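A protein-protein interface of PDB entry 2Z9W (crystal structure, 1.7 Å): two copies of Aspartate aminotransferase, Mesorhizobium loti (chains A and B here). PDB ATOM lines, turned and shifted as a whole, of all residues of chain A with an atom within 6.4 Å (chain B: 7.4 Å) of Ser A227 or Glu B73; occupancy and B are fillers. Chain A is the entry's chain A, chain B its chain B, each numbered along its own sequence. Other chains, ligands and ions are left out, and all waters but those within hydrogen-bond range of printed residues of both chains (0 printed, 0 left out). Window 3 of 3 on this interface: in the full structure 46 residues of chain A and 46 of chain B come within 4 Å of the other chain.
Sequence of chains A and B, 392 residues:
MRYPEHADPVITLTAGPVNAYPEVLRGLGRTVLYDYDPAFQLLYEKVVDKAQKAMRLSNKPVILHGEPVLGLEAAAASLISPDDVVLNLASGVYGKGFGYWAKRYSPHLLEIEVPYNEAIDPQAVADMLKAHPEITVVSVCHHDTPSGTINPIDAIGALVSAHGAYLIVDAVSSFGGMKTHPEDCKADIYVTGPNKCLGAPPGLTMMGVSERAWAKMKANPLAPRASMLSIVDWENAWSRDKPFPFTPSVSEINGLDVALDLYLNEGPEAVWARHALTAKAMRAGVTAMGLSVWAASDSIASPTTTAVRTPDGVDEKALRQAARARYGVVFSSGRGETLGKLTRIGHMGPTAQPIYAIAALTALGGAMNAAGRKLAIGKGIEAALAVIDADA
O of Arg A225 sits at hydrogen-bond distance from NH2 of Arg B104, 3.0 Å away. The indole nitrogen (NE1) of Trp B101 sits at hydrogen-bond distance from the backbone carbonyl oxygen (O) of Ala A226 (2.9 Å). The guanidinium group of Arg B104 lies within hydrogen-bond range of the backbone carbonyl oxygen of Ala A226 (2.9 Å). The side-chain hydroxyl (OG) of Ser A227 sits at hydrogen-bond distance from the side-chain carboxylate (OE2) of Glu B73, 2.6 Å away. The side-chain carboxylate (OE1) of Glu B73 lies within hydrogen-bond range of the backbone NH (N) of Met A228 (2.8 Å).
The side-chain carboxylate (OD1) of Asp A233 is in hydrogen-bond range of the backbone NH (N) of Ala A226 (2.6 Å). OG of Ser A227 sits close to N of Leu A229 (3.1 Å).
Among the printed residues, pairs that only touch across the chains: Met A228 with Val B69 (3.4 Å), Met A228 with Leu B70 (3.9 Å) and Phe A246 with Val B69 (3.7 Å).
Pro A224 touches none of the printed residues of chain B. Of the printed residues of chain B, Arg A225 touches Arg B104. Of the printed residues of chain B, Ala A226 touches Trp B101 (2.9 Å) and Arg B104 (2.9 Å). Ser A227 touches one residue of chain B. Of the printed residues of chain A, Leu B70 touches Met A228. Glu B73 touches two residues of chain A. Printed residues of chain A within 4 Å of Arg B104: Arg A225 and Ala A226. The nearest printed residue of chain B that does not touch Phe A246 is Leu B70 (6.5 Å).
Hydrophobic or aromatic side chains of chain A within 4 Å of the printed part of chain B: Ala A226, Met A228 and Phe A246. Hydrophobic or aromatic side chains of chain B that line the printed part of chain A: Val B69 and Trp B101. Along chain B the printed residues that touch a printed residue of chain A span positions 69 to 104. Among the printed residues, no Asp or Glu carboxylate lies within 4 Å of a Lys or Arg side-chain nitrogen of the other chain.
Positions printed for both chains: 224, 229 and 231. Of the 8 pairs that touch across the chains among the printed residues, none has its exchanged pair printed and touching as well.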
ATOM      1  N   PRO A 224      -9.238  -1.639 -19.666  1.00  0.00           N
ATOM      2  CA  PRO A 224     -10.063  -0.483 -19.282  1.00  0.00           C
ATOM      3  C   PRO A 224     -10.418  -0.408 -17.801  1.00  0.00           C
ATOM      4  O   PRO A 224     -10.799  -1.419 -17.169  1.00  0.00           O
ATOM      5  CB  PRO A 224     -11.316  -0.640 -20.148  1.00  0.00           C
ATOM      6  CG  PRO A 224     -10.829  -1.341 -21.368  1.00  0.00           C
ATOM      7  CD  PRO A 224      -9.754  -2.309 -20.876  1.00  0.00           C
ATOM      8  N   ARG A 225     -10.270   0.804 -17.260  1.00  0.00           N
ATOM      9  CA  ARG A 225     -10.626   1.134 -15.894  1.00  0.00           C
ATOM     10  C   ARG A 225     -11.245   2.525 -15.964  1.00  0.00           C
ATOM     11  O   ARG A 225     -10.865   3.318 -16.839  1.00  0.00           O
ATOM     12  CB  ARG A 225      -9.389   1.142 -14.999  1.00  0.00           C
ATOM     13  CG  ARG A 225      -8.773  -0.231 -14.804  1.00  0.00           C
ATOM     14  CD  ARG A 225      -7.411  -0.168 -14.083  1.00  0.00           C
ATOM     15  NE  ARG A 225      -6.940  -1.522 -13.780  1.00  0.00           N
ATOM     16  CZ  ARG A 225      -6.200  -2.284 -14.590  1.00  0.00           C
ATOM     17  NH1 ARG A 225      -5.850  -3.508 -14.192  1.00  0.00           N
ATOM     18  NH2 ARG A 225      -5.808  -1.847 -15.782  1.00  0.00           N
ATOM     19  N   ALA A 226     -12.220   2.789 -15.092  1.00  0.00           N
ATOM     20  CA  ALA A 226     -12.994   4.038 -15.139  1.00  0.00           C
ATOM     21  C   ALA A 226     -13.561   4.205 -16.548  1.00  0.00           C
ATOM     22  O   ALA A 226     -13.314   5.195 -17.230  1.00  0.00           O
ATOM     23  CB  ALA A 226     -12.118   5.230 -14.735  1.00  0.00           C
ATOM     24  N   SER A 227     -14.302   3.185 -16.991  1.00  0.00           N
ATOM     25  CA  SER A 227     -14.783   3.118 -18.356  1.00  0.00           C
ATOM     26  C   SER A 227     -15.958   2.153 -18.441  1.00  0.00           C
ATOM     27  O   SER A 227     -16.006   1.168 -17.700  1.00  0.00           O
ATOM     28  CB  SER A 227     -13.659   2.600 -19.262  1.00  0.00           C
ATOM     29  OG  SER A 227     -14.091   2.480 -20.598  1.00  0.00           O
ATOM     30  N   MET A 228     -16.877   2.409 -19.368  1.00  0.00           N
ATOM     31  CA  MET A 228     -17.964   1.468 -19.642  1.00  0.00           C
ATOM     32  C   MET A 228     -17.392   0.132 -20.111  1.00  0.00           C
ATOM     33  O   MET A 228     -18.041  -0.901 -19.944  1.00  0.00           O
ATOM     34  CB  MET A 228     -18.932   2.002 -20.711  1.00  0.00           C
ATOM     35  CG  MET A 228     -20.212   1.168 -20.815  1.00  0.00           C
ATOM     36  SD  MET A 228     -21.639   1.904 -19.987  1.00  0.00           S
ATOM     37  CE  MET A 228     -20.866   3.122 -18.962  1.00  0.00           C
ATOM     38  N   LEU A 229     -16.185   0.163 -20.685  1.00  0.00           N
ATOM     39  CA  LEU A 229     -15.510  -1.066 -21.124  1.00  0.00           C
ATOM     40  C   LEU A 229     -14.797  -1.840 -20.013  1.00  0.00           C
ATOM     41  O   LEU A 229     -14.198  -2.884 -20.288  1.00  0.00           O
ATOM     42  CB  LEU A 229     -14.515  -0.790 -22.262  1.00  0.00           C
ATOM     43  CG  LEU A 229     -15.032  -0.057 -23.496  1.00  0.00           C
ATOM     44  CD1 LEU A 229     -13.896   0.076 -24.520  1.00  0.00           C
ATOM     45  CD2 LEU A 229     -16.224  -0.772 -24.097  1.00  0.00           C
ATOM     46  N   SER A 230     -14.866  -1.364 -18.779  1.00  0.00           N
ATOM     47  CA  SER A 230     -14.125  -2.022 -17.701  1.00  0.00           C
ATOM     48  C   SER A 230     -14.833  -3.263 -17.169  1.00  0.00           C
ATOM     49  O   SER A 230     -15.979  -3.198 -16.747  1.00  0.00           O
ATOM     50  CB  SER A 230     -13.870  -1.072 -16.538  1.00  0.00           C
ATOM     51  OG  SER A 230     -13.011  -1.699 -15.603  1.00  0.00           O
ATOM     52  N   ILE A 231     -14.116  -4.392 -17.180  1.00  0.00           N
ATOM     53  CA  ILE A 231     -14.526  -5.582 -16.451  1.00  0.00           C
ATOM     54  C   ILE A 231     -13.963  -5.522 -15.029  1.00  0.00           C
ATOM     55  O   ILE A 231     -14.655  -5.806 -14.064  1.00  0.00           O
ATOM     56  CB  ILE A 231     -13.989  -6.860 -17.162  1.00  0.00           C
ATOM     57  CG1 ILE A 231     -14.584  -6.964 -18.570  1.00  0.00           C
ATOM     58  CG2 ILE A 231     -14.269  -8.120 -16.325  1.00  0.00           C
ATOM     59  CD1 ILE A 231     -13.844  -7.924 -19.505  1.00  0.00           C
ATOM     60  N   ASP A 233     -13.192  -3.167 -12.936  1.00  0.00           N
ATOM     61  CA  ASP A 233     -13.893  -2.281 -12.009  1.00  0.00           C
ATOM     62  C   ASP A 233     -15.111  -2.944 -11.355  1.00  0.00           C
ATOM     63  O   ASP A 233     -15.496  -2.566 -10.255  1.00  0.00           O
ATOM     64  CB  ASP A 233     -14.330  -0.998 -12.717  1.00  0.00           C
ATOM     65  CG  ASP A 233     -13.169  -0.037 -12.981  1.00  0.00           C
ATOM     66  OD1 ASP A 233     -13.451   1.028 -13.546  1.00  0.00           O
ATOM     67  OD2 ASP A 233     -12.006  -0.335 -12.624  1.00  0.00           O
ATOM     68  N   TRP A 234     -15.701  -3.930 -12.039  1.00  0.00           N
ATOM     69  CA  TRP A 234     -16.900  -4.628 -11.552  1.00  0.00           C
ATOM     70  C   TRP A 234     -16.605  -5.881 -10.719  1.00  0.00           C
ATOM     71  O   TRP A 234     -17.528  -6.601 -10.309  1.00  0.00           O
ATOM     72  CB  TRP A 234     -17.850  -4.938 -12.722  1.00  0.00           C
ATOM     73  CG  TRP A 234     -18.520  -3.673 -13.196  1.00  0.00           C
ATOM     74  CD1 TRP A 234     -17.989  -2.730 -14.043  1.00  0.00           C
ATOM     75  CD2 TRP A 234     -19.808  -3.169 -12.799  1.00  0.00           C
ATOM     76  NE1 TRP A 234     -18.864  -1.689 -14.198  1.00  0.00           N
ATOM     77  CE2 TRP A 234     -19.988  -1.925 -13.452  1.00  0.00           C
ATOM     78  CE3 TRP A 234     -20.827  -3.645 -11.961  1.00  0.00           C
ATOM     79  CZ2 TRP A 234     -21.157  -1.155 -13.305  1.00  0.00           C
ATOM     80  CZ3 TRP A 234     -21.995  -2.874 -11.810  1.00  0.00           C
ATOM     81  CH2 TRP A 234     -22.142  -1.639 -12.484  1.00  0.00           C
ATOM     82  N   PHE A 246     -20.748   2.373 -11.726  1.00  0.00           N
ATOM     83  CA  PHE A 246     -21.750   3.366 -12.145  1.00  0.00           C
ATOM     84  C   PHE A 246     -23.133   2.757 -11.912  1.00  0.00           C
ATOM     85  O   PHE A 246     -23.242   1.573 -11.524  1.00  0.00           O
ATOM     86  CB  PHE A 246     -21.547   3.813 -13.609  1.00  0.00           C
ATOM     87  CG  PHE A 246     -21.643   2.689 -14.627  1.00  0.00           C
ATOM     88  CD1 PHE A 246     -20.482   2.047 -15.084  1.00  0.00           C
ATOM     89  CD2 PHE A 246     -22.884   2.314 -15.159  1.00  0.00           C
ATOM     90  CE1 PHE A 246     -20.549   1.020 -16.033  1.00  0.00           C
ATOM     91  CE2 PHE A 246     -22.975   1.295 -16.114  1.00  0.00           C
ATOM     92  CZ  PHE A 246     -21.806   0.638 -16.548  1.00  0.00           C
ATOM     93  N   PRO B  68     -26.280   7.424 -18.665  1.00  0.00           N
ATOM     94  CA  PRO B  68     -25.515   8.582 -19.133  1.00  0.00           C
ATOM     95  C   PRO B  68     -24.005   8.703 -18.873  1.00  0.00           C
ATOM     96  O   PRO B  68     -23.356   9.494 -19.575  1.00  0.00           O
ATOM     97  CB  PRO B  68     -26.286   9.771 -18.517  1.00  0.00           C
ATOM     98  CG  PRO B  68     -27.711   9.275 -18.466  1.00  0.00           C
ATOM     99  CD  PRO B  68     -27.529   7.832 -17.991  1.00  0.00           C
ATOM    100  N   VAL B  69     -23.429   7.970 -17.912  1.00  0.00           N
ATOM    101  CA  VAL B  69     -21.948   7.910 -17.843  1.00  0.00           C
ATOM    102  C   VAL B  69     -21.343   7.479 -19.177  1.00  0.00           C
ATOM    103  O   VAL B  69     -20.240   7.904 -19.518  1.00  0.00           O
ATOM    104  CB  VAL B  69     -21.392   6.994 -16.721  1.00  0.00           C
ATOM    105  CG1 VAL B  69     -21.651   7.612 -15.354  1.00  0.00           C
ATOM    106  CG2 VAL B  69     -21.965   5.584 -16.831  1.00  0.00           C
ATOM    107  N   LEU B  70     -22.076   6.660 -19.940  1.00  0.00           N
ATOM    108  CA  LEU B  70     -21.642   6.302 -21.298  1.00  0.00           C
ATOM    109  C   LEU B  70     -21.554   7.542 -22.186  1.00  0.00           C
ATOM    110  O   LEU B  70     -20.595   7.711 -22.926  1.00  0.00           O
ATOM    111  CB  LEU B  70     -22.622   5.317 -21.941  1.00  0.00           C
ATOM    112  CG  LEU B  70     -22.350   4.991 -23.421  1.00  0.00           C
ATOM    113  CD1 LEU B  70     -20.952   4.389 -23.592  1.00  0.00           C
ATOM    114  CD2 LEU B  70     -23.422   4.054 -23.978  1.00  0.00           C
ATOM    115  N   GLY B  71     -22.595   8.369 -22.138  1.00  0.00           N
ATOM    116  CA  GLY B  71     -22.620   9.609 -22.917  1.00  0.00           C
ATOM    117  C   GLY B  71     -21.448  10.507 -22.558  1.00  0.00           C
ATOM    118  O   GLY B  71     -20.816  11.104 -23.434  1.00  0.00           O
ATOM    119  N   LEU B  72     -21.149  10.604 -21.269  1.00  0.00           N
ATOM    120  CA  LEU B  72     -20.072  11.474 -20.811  1.00  0.00           C
ATOM    121  C   LEU B  72     -18.720  10.960 -21.284  1.00  0.00           C
ATOM    122  O   LEU B  72     -17.917  11.714 -21.825  1.00  0.00           O
ATOM    123  CB  LEU B  72     -20.096  11.615 -19.282  1.00  0.00           C
ATOM    124  CG  LEU B  72     -21.366  12.264 -18.703  1.00  0.00           C
ATOM    125  CD1 LEU B  72     -21.373  12.146 -17.193  1.00  0.00           C
ATOM    126  CD2 LEU B  72     -21.433  13.729 -19.146  1.00  0.00           C
ATOM    127  N   GLU B  73     -18.465   9.676 -21.054  1.00  0.00           N
ATOM    128  CA  GLU B  73     -17.226   9.071 -21.509  1.00  0.00           C
ATOM    129  C   GLU B  73     -17.083   9.139 -23.033  1.00  0.00           C
ATOM    130  O   GLU B  73     -16.013   9.481 -23.549  1.00  0.00           O
ATOM    131  CB  GLU B  73     -17.144   7.617 -21.054  1.00  0.00           C
ATOM    132  CG  GLU B  73     -15.783   6.994 -21.393  1.00  0.00           C
ATOM    133  CD  GLU B  73     -15.711   5.521 -21.044  1.00  0.00           C
ATOM    134  OE1 GLU B  73     -16.708   4.967 -20.515  1.00  0.00           O
ATOM    135  OE2 GLU B  73     -14.643   4.921 -21.316  1.00  0.00           O
ATOM    136  N   ALA B  74     -18.151   8.799 -23.750  1.00  0.00           N
ATOM    137  CA  ALA B  74     -18.145   8.814 -25.216  1.00  0.00           C
ATOM    138  C   ALA B  74     -17.911  10.231 -25.757  1.00  0.00           C
ATOM    139  O   ALA B  74     -17.217  10.403 -26.762  1.00  0.00           O
ATOM    140  CB  ALA B  74     -19.446   8.241 -25.761  1.00  0.00           C
ATOM    141  N   ALA B  75     -18.456  11.230 -25.072  1.00  0.00           N
ATOM    142  CA  ALA B  75     -18.237  12.624 -25.463  1.00  0.00           C
ATOM    143  C   ALA B  75     -16.772  13.026 -25.363  1.00  0.00           C
ATOM    144  O   ALA B  75     -16.203  13.588 -26.304  1.00  0.00           O
ATOM    145  CB  ALA B  75     -19.117  13.559 -24.646  1.00  0.00           C
ATOM    146  N   ALA B  76     -16.151  12.710 -24.230  1.00  0.00           N
ATOM    147  CA  ALA B  76     -14.723  12.972 -24.055  1.00  0.00           C
ATOM    148  C   ALA B  76     -13.920  12.222 -25.114  1.00  0.00           C
ATOM    149  O   ALA B  76     -13.045  12.793 -25.751  1.00  0.00           O
ATOM    150  CB  ALA B  76     -14.281  12.554 -22.686  1.00  0.00           C
ATOM    151  N   ALA B  77     -14.219  10.932 -25.295  1.00  0.00           N
ATOM    152  CA  ALA B  77     -13.431  10.096 -26.203  1.00  0.00           C
ATOM    153  C   ALA B  77     -13.513  10.524 -27.674  1.00  0.00           C
ATOM    154  O   ALA B  77     -12.560  10.313 -28.453  1.00  0.00           O
ATOM    155  CB  ALA B  77     -13.858   8.623 -26.054  1.00  0.00           C
ATOM    156  N   SER B  78     -14.647  11.119 -28.043  1.00  0.00           N
ATOM    157  CA  SER B  78     -14.930  11.472 -29.433  1.00  0.00           C
ATOM    158  C   SER B  78     -14.576  12.913 -29.796  1.00  0.00           C
ATOM    159  O   SER B  78     -14.075  13.185 -30.893  1.00  0.00           O
ATOM    160  CB  SER B  78     -16.415  11.253 -29.719  1.00  0.00           C
ATOM    161  OG  SER B  78     -16.795   9.906 -29.467  1.00  0.00           O
ATOM    162  N   LEU B  79     -14.902  13.832 -28.887  1.00  0.00           N
ATOM    163  CA  LEU B  79     -14.734  15.255 -29.158  1.00  0.00           C
ATOM    164  C   LEU B  79     -13.352  15.752 -28.770  1.00  0.00           C
ATOM    165  O   LEU B  79     -12.835  16.662 -29.417  1.00  0.00           O
ATOM    166  CB  LEU B  79     -15.821  16.083 -28.431  1.00  0.00           C
ATOM    167  CG  LEU B  79     -16.020  17.529 -28.923  1.00  0.00           C
ATOM    168  CD1 LEU B  79     -16.724  17.557 -30.299  1.00  0.00           C
ATOM    169  CD2 LEU B  79     -16.837  18.341 -27.894  1.00  0.00           C
ATOM    170  N   PHE B  98     -15.319  14.726 -14.634  1.00  0.00           N
ATOM    171  CA  PHE B  98     -15.227  14.817 -16.089  1.00  0.00           C
ATOM    172  C   PHE B  98     -13.791  15.140 -16.515  1.00  0.00           C
ATOM    173  O   PHE B  98     -13.323  14.671 -17.554  1.00  0.00           O
ATOM    174  CB  PHE B  98     -16.187  15.841 -16.692  1.00  0.00           C
ATOM    175  CG  PHE B  98     -16.268  15.729 -18.178  1.00  0.00           C
ATOM    176  CD1 PHE B  98     -15.411  16.473 -18.996  1.00  0.00           C
ATOM    177  CD2 PHE B  98     -17.165  14.843 -18.760  1.00  0.00           C
ATOM    178  CE1 PHE B  98     -15.462  16.323 -20.389  1.00  0.00           C
ATOM    179  CE2 PHE B  98     -17.227  14.687 -20.133  1.00  0.00           C
ATOM    180  CZ  PHE B  98     -16.383  15.423 -20.952  1.00  0.00           C
ATOM    181  N   TRP B 101     -11.662  12.179 -17.447  1.00  0.00           N
ATOM    182  CA  TRP B 101     -11.869  11.705 -18.806  1.00  0.00           C
ATOM    183  C   TRP B 101     -11.265  12.662 -19.831  1.00  0.00           C
ATOM    184  O   TRP B 101     -10.674  12.231 -20.824  1.00  0.00           O
ATOM    185  CB  TRP B 101     -13.343  11.447 -19.098  1.00  0.00           C
ATOM    186  CG  TRP B 101     -13.839  10.123 -18.594  1.00  0.00           C
ATOM    187  CD1 TRP B 101     -13.129   8.937 -18.508  1.00  0.00           C
ATOM    188  CD2 TRP B 101     -15.162   9.827 -18.156  1.00  0.00           C
ATOM    189  NE1 TRP B 101     -13.937   7.941 -18.012  1.00  0.00           N
ATOM    190  CE2 TRP B 101     -15.192   8.453 -17.801  1.00  0.00           C
ATOM    191  CE3 TRP B 101     -16.326  10.592 -18.002  1.00  0.00           C
ATOM    192  CZ2 TRP B 101     -16.343   7.834 -17.296  1.00  0.00           C
ATOM    193  CZ3 TRP B 101     -17.470   9.974 -17.509  1.00  0.00           C
ATOM    194  CH2 TRP B 101     -17.470   8.603 -17.165  1.00  0.00           C
ATOM    195  N   ARG B 104      -7.642  11.909 -20.091  1.00  0.00           N
ATOM    196  CA  ARG B 104      -7.398  10.648 -20.791  1.00  0.00           C
ATOM    197  C   ARG B 104      -7.239  10.888 -22.297  1.00  0.00           C
ATOM    198  O   ARG B 104      -6.505  10.155 -22.975  1.00  0.00           O
ATOM    199  CB  ARG B 104      -8.532   9.651 -20.534  1.00  0.00           C
ATOM    200  CG  ARG B 104      -8.458   8.378 -21.382  1.00  0.00           C
ATOM    201  CD  ARG B 104      -9.481   7.369 -20.897  1.00  0.00           C
ATOM    202  NE  ARG B 104      -9.121   6.894 -19.558  1.00  0.00           N
ATOM    203  CZ  ARG B 104      -9.910   6.190 -18.742  1.00  0.00           C
ATOM    204  NH1 ARG B 104     -11.151   5.861 -19.096  1.00  0.00           N
ATOM    205  NH2 ARG B 104      -9.439   5.808 -17.555  1.00  0.00           N
ATOM    206  N   TYR B 105      -7.891  11.934 -22.809  1.00  0.00           N
ATOM    207  CA  TYR B 105      -7.986  12.149 -24.264  1.00  0.00           C
ATOM    208  C   TYR B 105      -7.231  13.373 -24.781  1.00  0.00           C
ATOM    209  O   TYR B 105      -7.046  13.543 -25.998  1.00  0.00           O
ATOM    210  CB  TYR B 105      -9.465  12.164 -24.698  1.00  0.00           C
ATOM    211  CG  TYR B 105     -10.081  10.803 -24.493  1.00  0.00           C
ATOM    212  CD1 TYR B 105      -9.718   9.751 -25.314  1.00  0.00           C
ATOM    213  CD2 TYR B 105     -10.992  10.554 -23.461  1.00  0.00           C
ATOM    214  CE1 TYR B 105     -10.245   8.486 -25.136  1.00  0.00           C
ATOM    215  CE2 TYR B 105     -11.539   9.274 -23.270  1.00  0.00           C
ATOM    216  CZ  TYR B 105     -11.148   8.247 -24.127  1.00  0.00           C
ATOM    217  OH  TYR B 105     -11.649   6.963 -24.006  1.00  0.00           O
ATOM    218  N   VAL B 191     -25.417  16.192 -22.618  1.00  0.00           N
ATOM    219  CA  VAL B 191     -25.687  14.822 -22.173  1.00  0.00           C
ATOM    220  C   VAL B 191     -26.768  14.833 -21.111  1.00  0.00           C
ATOM    221  O   VAL B 191     -26.641  15.511 -20.080  1.00  0.00           O
ATOM    222  CB  VAL B 191     -24.410  14.124 -21.607  1.00  0.00           C
ATOM    223  CG1 VAL B 191     -24.713  12.684 -21.137  1.00  0.00           C
ATOM    224  CG2 VAL B 191     -23.254  14.167 -22.639  1.00  0.00           C
ATOM    225  N   MET B 207     -28.646  12.518 -26.053  1.00  0.00           N
ATOM    226  CA  MET B 207     -27.517  13.408 -26.303  1.00  0.00           C
ATOM    227  C   MET B 207     -27.783  14.418 -27.405  1.00  0.00           C
ATOM    228  O   MET B 207     -28.021  14.047 -28.550  1.00  0.00           O
ATOM    229  CB  MET B 207     -26.266  12.583 -26.629  1.00  0.00           C
ATOM    230  CG  MET B 207     -25.026  13.454 -26.838  1.00  0.00           C
ATOM    231  SD  MET B 207     -23.585  12.517 -27.432  1.00  0.00           S
ATOM    232  CE  MET B 207     -23.039  11.772 -25.894  1.00  0.00           C
ATOM    233  N   PRO B 224     -14.006   6.913 -30.991  1.00  0.00           N
ATOM    234  CA  PRO B 224     -14.444   5.510 -31.040  1.00  0.00           C
ATOM    235  C   PRO B 224     -15.394   5.201 -32.204  1.00  0.00           C
ATOM    236  O   PRO B 224     -16.348   5.968 -32.456  1.00  0.00           O
ATOM    237  CB  PRO B 224     -15.148   5.310 -29.685  1.00  0.00           C
ATOM    238  CG  PRO B 224     -14.443   6.287 -28.772  1.00  0.00           C
ATOM    239  CD  PRO B 224     -14.237   7.514 -29.664  1.00  0.00           C
ATOM    240  N   LEU B 229     -18.444   2.874 -27.023  1.00  0.00           N
ATOM    241  CA  LEU B 229     -18.151   4.279 -26.771  1.00  0.00           C
ATOM    242  C   LEU B 229     -18.366   5.160 -27.992  1.00  0.00           C
ATOM    243  O   LEU B 229     -18.066   6.355 -27.936  1.00  0.00           O
ATOM    244  CB  LEU B 229     -16.711   4.458 -26.269  1.00  0.00           C
ATOM    245  CG  LEU B 229     -16.310   3.710 -24.999  1.00  0.00           C
ATOM    246  CD1 LEU B 229     -14.858   3.997 -24.677  1.00  0.00           C
ATOM    247  CD2 LEU B 229     -17.204   4.121 -23.840  1.00  0.00           C
ATOM    248  N   ILE B 231     -20.163   7.491 -30.574  1.00  0.00           N
ATOM    249  CA  ILE B 231     -21.271   8.365 -30.930  1.00  0.00           C
ATOM    250  C   ILE B 231     -21.451   8.352 -32.446  1.00  0.00           C
ATOM    251  O   ILE B 231     -22.569   8.264 -32.952  1.00  0.00           O
ATOM    252  CB  ILE B 231     -21.035   9.813 -30.408  1.00  0.00           C
ATOM    253  CG1 ILE B 231     -20.930   9.786 -28.888  1.00  0.00           C
ATOM    254  CG2 ILE B 231     -22.153  10.746 -30.872  1.00  0.00           C
ATOM    255  CD1 ILE B 231     -20.271  11.051 -28.271  1.00  0.00           C
